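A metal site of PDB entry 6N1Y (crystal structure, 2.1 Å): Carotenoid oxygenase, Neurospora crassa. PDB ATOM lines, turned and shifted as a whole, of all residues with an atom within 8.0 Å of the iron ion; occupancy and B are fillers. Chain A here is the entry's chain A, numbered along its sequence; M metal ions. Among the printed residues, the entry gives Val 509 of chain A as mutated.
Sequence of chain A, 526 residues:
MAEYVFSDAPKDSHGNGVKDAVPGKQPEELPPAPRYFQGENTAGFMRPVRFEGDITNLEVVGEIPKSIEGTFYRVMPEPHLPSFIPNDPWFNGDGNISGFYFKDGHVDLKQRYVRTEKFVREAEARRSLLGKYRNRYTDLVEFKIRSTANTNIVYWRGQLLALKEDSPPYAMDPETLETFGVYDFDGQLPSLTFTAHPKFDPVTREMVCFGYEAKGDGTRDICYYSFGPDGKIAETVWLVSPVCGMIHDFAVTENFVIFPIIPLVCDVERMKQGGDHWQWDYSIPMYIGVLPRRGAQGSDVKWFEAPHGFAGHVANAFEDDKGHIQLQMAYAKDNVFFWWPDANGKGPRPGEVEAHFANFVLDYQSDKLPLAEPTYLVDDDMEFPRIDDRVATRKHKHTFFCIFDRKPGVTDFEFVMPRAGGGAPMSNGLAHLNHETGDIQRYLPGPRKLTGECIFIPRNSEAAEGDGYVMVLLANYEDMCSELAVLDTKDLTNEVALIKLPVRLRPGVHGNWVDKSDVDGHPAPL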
ATOM      1  N   THR A 151     -26.631   7.195 -13.585  1.00  0.00           N
ATOM      2  CA  THR A 151     -26.149   6.638 -14.880  1.00  0.00           C
ATOM      3  C   THR A 151     -24.726   7.120 -15.182  1.00  0.00           C
ATOM      4  O   THR A 151     -23.891   6.272 -15.545  1.00  0.00           O
ATOM      5  CB  THR A 151     -27.106   6.987 -16.036  1.00  0.00           C
ATOM      6  OG1 THR A 151     -28.411   6.566 -15.644  1.00  0.00           O
ATOM      7  CG2 THR A 151     -26.720   6.325 -17.333  1.00  0.00           C
ATOM      8  N   ASN A 152     -24.462   8.410 -15.079  1.00  0.00           N
ATOM      9  CA  ASN A 152     -23.131   8.977 -15.416  1.00  0.00           C
ATOM     10  C   ASN A 152     -22.856  10.162 -14.491  1.00  0.00           C
ATOM     11  O   ASN A 152     -23.809  10.746 -13.957  1.00  0.00           O
ATOM     12  CB  ASN A 152     -23.056   9.368 -16.904  1.00  0.00           C
ATOM     13  CG  ASN A 152     -21.640   9.457 -17.431  1.00  0.00           C
ATOM     14  OD1 ASN A 152     -20.665   9.207 -16.711  1.00  0.00           O
ATOM     15  ND2 ASN A 152     -21.509   9.807 -18.699  1.00  0.00           N
ATOM     16  N   GLU A 165     -31.244  10.043 -17.927  1.00  0.00           N
ATOM     17  CA  GLU A 165     -31.724  10.518 -19.258  1.00  0.00           C
ATOM     18  C   GLU A 165     -33.209  10.911 -19.227  1.00  0.00           C
ATOM     19  O   GLU A 165     -33.674  11.502 -20.223  1.00  0.00           O
ATOM     20  CB  GLU A 165     -31.444   9.451 -20.331  1.00  0.00           C
ATOM     21  CG  GLU A 165     -32.258   8.186 -20.184  1.00  0.00           C
ATOM     22  CD  GLU A 165     -31.676   6.975 -20.903  1.00  0.00           C
ATOM     23  OE1 GLU A 165     -32.423   6.303 -21.629  1.00  0.00           O
ATOM     24  OE2 GLU A 165     -30.483   6.697 -20.701  1.00  0.00           O
ATOM     25  N   THR A 195     -29.387  13.834 -21.682  1.00  0.00           N
ATOM     26  CA  THR A 195     -28.745  12.518 -21.939  1.00  0.00           C
ATOM     27  C   THR A 195     -27.694  12.209 -20.870  1.00  0.00           C
ATOM     28  O   THR A 195     -27.045  13.153 -20.381  1.00  0.00           O
ATOM     29  CB  THR A 195     -28.090  12.463 -23.329  1.00  0.00           C
ATOM     30  OG1 THR A 195     -27.551  11.155 -23.516  1.00  0.00           O
ATOM     31  CG2 THR A 195     -26.981  13.480 -23.510  1.00  0.00           C
ATOM     32  N   ALA A 196     -27.487  10.937 -20.563  1.00  0.00           N
ATOM     33  CA  ALA A 196     -26.402  10.441 -19.698  1.00  0.00           C
ATOM     34  C   ALA A 196     -25.067  10.422 -20.455  1.00  0.00           C
ATOM     35  O   ALA A 196     -24.025  10.152 -19.823  1.00  0.00           O
ATOM     36  CB  ALA A 196     -26.746   9.073 -19.170  1.00  0.00           C
ATOM     37  N   HIS A 197     -25.074  10.682 -21.771  1.00  0.00           N
ATOM     38  CA  HIS A 197     -23.880  10.540 -22.633  1.00  0.00           C
ATOM     39  C   HIS A 197     -23.668  11.799 -23.460  1.00  0.00           C
ATOM     40  O   HIS A 197     -23.642  11.742 -24.683  1.00  0.00           O
ATOM     41  CB  HIS A 197     -24.003   9.257 -23.463  1.00  0.00           C
ATOM     42  CG  HIS A 197     -23.871   8.027 -22.639  1.00  0.00           C
ATOM     43  ND1 HIS A 197     -22.675   7.659 -22.055  1.00  0.00           N
ATOM     44  CD2 HIS A 197     -24.776   7.079 -22.273  1.00  0.00           C
ATOM     45  CE1 HIS A 197     -22.837   6.552 -21.360  1.00  0.00           C
ATOM     46  NE2 HIS A 197     -24.125   6.159 -21.484  1.00  0.00           N
ATOM     47  N   HIS A 248     -30.324   6.142 -25.877  1.00  0.00           N
ATOM     48  CA  HIS A 248     -29.455   6.097 -24.666  1.00  0.00           C
ATOM     49  C   HIS A 248     -28.161   6.884 -24.932  1.00  0.00           C
ATOM     50  O   HIS A 248     -27.750   7.667 -24.056  1.00  0.00           O
ATOM     51  CB  HIS A 248     -29.127   4.669 -24.252  1.00  0.00           C
ATOM     52  CG  HIS A 248     -28.218   4.626 -23.065  1.00  0.00           C
ATOM     53  ND1 HIS A 248     -28.634   5.059 -21.828  1.00  0.00           N
ATOM     54  CD2 HIS A 248     -26.930   4.254 -22.916  1.00  0.00           C
ATOM     55  CE1 HIS A 248     -27.654   4.949 -20.961  1.00  0.00           C
ATOM     56  NE2 HIS A 248     -26.601   4.450 -21.601  1.00  0.00           N
ATOM     57  N   ASP A 249     -27.531   6.617 -26.076  1.00  0.00           N
ATOM     58  CA  ASP A 249     -26.244   7.230 -26.464  1.00  0.00           C
ATOM     59  C   ASP A 249     -26.437   7.956 -27.795  1.00  0.00           C
ATOM     60  O   ASP A 249     -27.471   7.735 -28.430  1.00  0.00           O
ATOM     61  CB  ASP A 249     -25.147   6.160 -26.521  1.00  0.00           C
ATOM     62  CG  ASP A 249     -23.754   6.685 -26.260  1.00  0.00           C
ATOM     63  OD1 ASP A 249     -23.543   7.913 -26.407  1.00  0.00           O
ATOM     64  OD2 ASP A 249     -22.883   5.854 -25.915  1.00  0.00           O
ATOM     65  N   GLY A 312     -25.970  -0.258 -28.730  1.00  0.00           N
ATOM     66  CA  GLY A 312     -25.156  -0.156 -27.504  1.00  0.00           C
ATOM     67  C   GLY A 312     -24.429   1.179 -27.412  1.00  0.00           C
ATOM     68  O   GLY A 312     -24.770   2.094 -28.187  1.00  0.00           O
ATOM     69  N   HIS A 313     -23.455   1.291 -26.511  1.00  0.00           N
ATOM     70  CA  HIS A 313     -22.674   2.533 -26.268  1.00  0.00           C
ATOM     71  C   HIS A 313     -21.819   2.860 -27.488  1.00  0.00           C
ATOM     72  O   HIS A 313     -21.219   1.933 -28.076  1.00  0.00           O
ATOM     73  CB  HIS A 313     -21.852   2.408 -24.985  1.00  0.00           C
ATOM     74  CG  HIS A 313     -22.669   2.495 -23.743  1.00  0.00           C
ATOM     75  ND1 HIS A 313     -22.902   1.404 -22.939  1.00  0.00           N
ATOM     76  CD2 HIS A 313     -23.327   3.535 -23.197  1.00  0.00           C
ATOM     77  CE1 HIS A 313     -23.685   1.772 -21.935  1.00  0.00           C
ATOM     78  NE2 HIS A 313     -23.949   3.068 -22.069  1.00  0.00           N
ATOM     79  N   VAL A 314     -21.767   4.130 -27.859  1.00  0.00           N
ATOM     80  CA  VAL A 314     -20.890   4.695 -28.917  1.00  0.00           C
ATOM     81  C   VAL A 314     -19.464   4.799 -28.368  1.00  0.00           C
ATOM     82  O   VAL A 314     -19.272   5.420 -27.309  1.00  0.00           O
ATOM     83  CB  VAL A 314     -21.412   6.075 -29.373  1.00  0.00           C
ATOM     84  CG1 VAL A 314     -20.448   6.741 -30.349  1.00  0.00           C
ATOM     85  CG2 VAL A 314     -22.813   5.981 -29.953  1.00  0.00           C
ATOM     86  N   PHE A 337     -31.778  -5.671 -23.181  1.00  0.00           N
ATOM     87  CA  PHE A 337     -32.663  -5.407 -22.024  1.00  0.00           C
ATOM     88  C   PHE A 337     -33.864  -6.376 -22.069  1.00  0.00           C
ATOM     89  O   PHE A 337     -35.020  -5.927 -22.260  1.00  0.00           O
ATOM     90  CB  PHE A 337     -33.086  -3.932 -21.987  1.00  0.00           C
ATOM     91  CG  PHE A 337     -31.950  -2.928 -21.893  1.00  0.00           C
ATOM     92  CD1 PHE A 337     -30.666  -3.320 -21.555  1.00  0.00           C
ATOM     93  CD2 PHE A 337     -32.188  -1.586 -22.130  1.00  0.00           C
ATOM     94  CE1 PHE A 337     -29.637  -2.386 -21.487  1.00  0.00           C
ATOM     95  CE2 PHE A 337     -31.172  -0.660 -22.043  1.00  0.00           C
ATOM     96  CZ  PHE A 337     -29.893  -1.053 -21.729  1.00  0.00           C
ATOM     97  N   GLU A 383     -18.701  -4.330 -24.470  1.00  0.00           N
ATOM     98  CA  GLU A 383     -19.501  -3.116 -24.161  1.00  0.00           C
ATOM     99  C   GLU A 383     -18.589  -2.104 -23.444  1.00  0.00           C
ATOM    100  O   GLU A 383     -17.406  -2.420 -23.217  1.00  0.00           O
ATOM    101  CB  GLU A 383     -20.746  -3.463 -23.346  1.00  0.00           C
ATOM    102  CG  GLU A 383     -22.056  -3.239 -24.097  1.00  0.00           C
ATOM    103  CD  GLU A 383     -22.384  -1.786 -24.425  1.00  0.00           C
ATOM    104  OE1 GLU A 383     -21.656  -0.894 -23.962  1.00  0.00           O
ATOM    105  OE2 GLU A 383     -23.372  -1.547 -25.162  1.00  0.00           O
ATOM    106  N   PHE A 384     -19.130  -0.921 -23.135  1.00  0.00           N
ATOM    107  CA  PHE A 384     -18.468   0.143 -22.357  1.00  0.00           C
ATOM    108  C   PHE A 384     -17.168   0.566 -23.045  1.00  0.00           C
ATOM    109  O   PHE A 384     -16.109   0.568 -22.431  1.00  0.00           O
ATOM    110  CB  PHE A 384     -18.262  -0.306 -20.911  1.00  0.00           C
ATOM    111  CG  PHE A 384     -19.547  -0.544 -20.155  1.00  0.00           C
ATOM    112  CD1 PHE A 384     -20.367   0.523 -19.832  1.00  0.00           C
ATOM    113  CD2 PHE A 384     -19.944  -1.832 -19.798  1.00  0.00           C
ATOM    114  CE1 PHE A 384     -21.557   0.314 -19.145  1.00  0.00           C
ATOM    115  CE2 PHE A 384     -21.130  -2.028 -19.104  1.00  0.00           C
ATOM    116  CZ  PHE A 384     -21.927  -0.961 -18.782  1.00  0.00           C
ATOM    117  N   GLU A 453     -16.639  -0.403 -16.007  1.00  0.00           N
ATOM    118  CA  GLU A 453     -16.138   0.454 -17.118  1.00  0.00           C
ATOM    119  C   GLU A 453     -14.792   1.040 -16.708  1.00  0.00           C
ATOM    120  O   GLU A 453     -14.655   1.491 -15.553  1.00  0.00           O
ATOM    121  CB  GLU A 453     -17.154   1.556 -17.437  1.00  0.00           C
ATOM    122  CG  GLU A 453     -16.719   2.460 -18.561  1.00  0.00           C
ATOM    123  CD  GLU A 453     -17.487   3.776 -18.617  1.00  0.00           C
ATOM    124  OE1 GLU A 453     -17.427   4.530 -17.620  1.00  0.00           O
ATOM    125  OE2 GLU A 453     -18.134   4.027 -19.664  1.00  0.00           O
ATOM    126  N   VAL A 509     -22.064   2.037 -13.053  1.00  0.00           N
ATOM    127  CA  VAL A 509     -22.313   2.335 -14.486  1.00  0.00           C
ATOM    128  C   VAL A 509     -21.083   3.099 -14.988  1.00  0.00           C
ATOM    129  O   VAL A 509     -19.991   2.509 -14.942  1.00  0.00           O
ATOM    130  CB  VAL A 509     -23.647   3.085 -14.665  1.00  0.00           C
ATOM    131  CG1 VAL A 509     -24.120   3.065 -16.119  1.00  0.00           C
ATOM    132  CG2 VAL A 509     -24.727   2.524 -13.758  1.00  0.00           C
ATOM    133  N   HIS A 510     -21.233   4.357 -15.402  1.00  0.00           N
ATOM    134  CA  HIS A 510     -20.159   5.139 -16.050  1.00  0.00           C
ATOM    135  C   HIS A 510     -19.331   5.892 -14.993  1.00  0.00           C
ATOM    136  O   HIS A 510     -19.808   6.088 -13.856  1.00  0.00           O
ATOM    137  CB  HIS A 510     -20.773   6.042 -17.124  1.00  0.00           C
ATOM    138  CG  HIS A 510     -21.496   5.263 -18.179  1.00  0.00           C
ATOM    139  ND1 HIS A 510     -20.840   4.490 -19.101  1.00  0.00           N
ATOM    140  CD2 HIS A 510     -22.816   5.115 -18.431  1.00  0.00           C
ATOM    141  CE1 HIS A 510     -21.716   3.896 -19.887  1.00  0.00           C
ATOM    142  NE2 HIS A 510     -22.938   4.267 -19.495  1.00  0.00           N
HETATM  143 FE    FE M   1     -24.758   4.340 -20.644  1.00  0.00          FE
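Four residues have an atom within 4 Å of the iron ion: His 197, His 248, His 313 and His 510. The nearest printed residue that does not touch the iron ion is Thr 151 (4.3 Å).
The iron ion is bound by NE2 of His 313 (2.1 Å). The iron ion is bound by NE2 of His 248. A ring nitrogen (NE2) of His 197 binds the iron ion. The iron ion is bound by NE2 of His 510, 2.2 Å away.
A ring nitrogen (ND1) of His 313 sits at hydrogen-bond distance from the side-chain carboxylate (OE1) of Glu 383, at 2.8 Å. A ring nitrogen (ND1) of His 248 is in hydrogen-bond range of the side-chain carboxylate (OE2) of Glu 165. The backbone NH (N) of His 197 sits at hydrogen-bond distance from the side-chain hydroxyl (OG1) of Thr 195, at 3.1 Å. The backbone NH (N) of His 510 lies within hydrogen-bond range of the backbone carbonyl oxygen (O) of Thr 151, at 3.3 Å. A ring nitrogen (ND1) of His 510 lies within hydrogen-bond range of the side-chain carboxylate (OE2) of Glu 453, at 2.8 Å.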
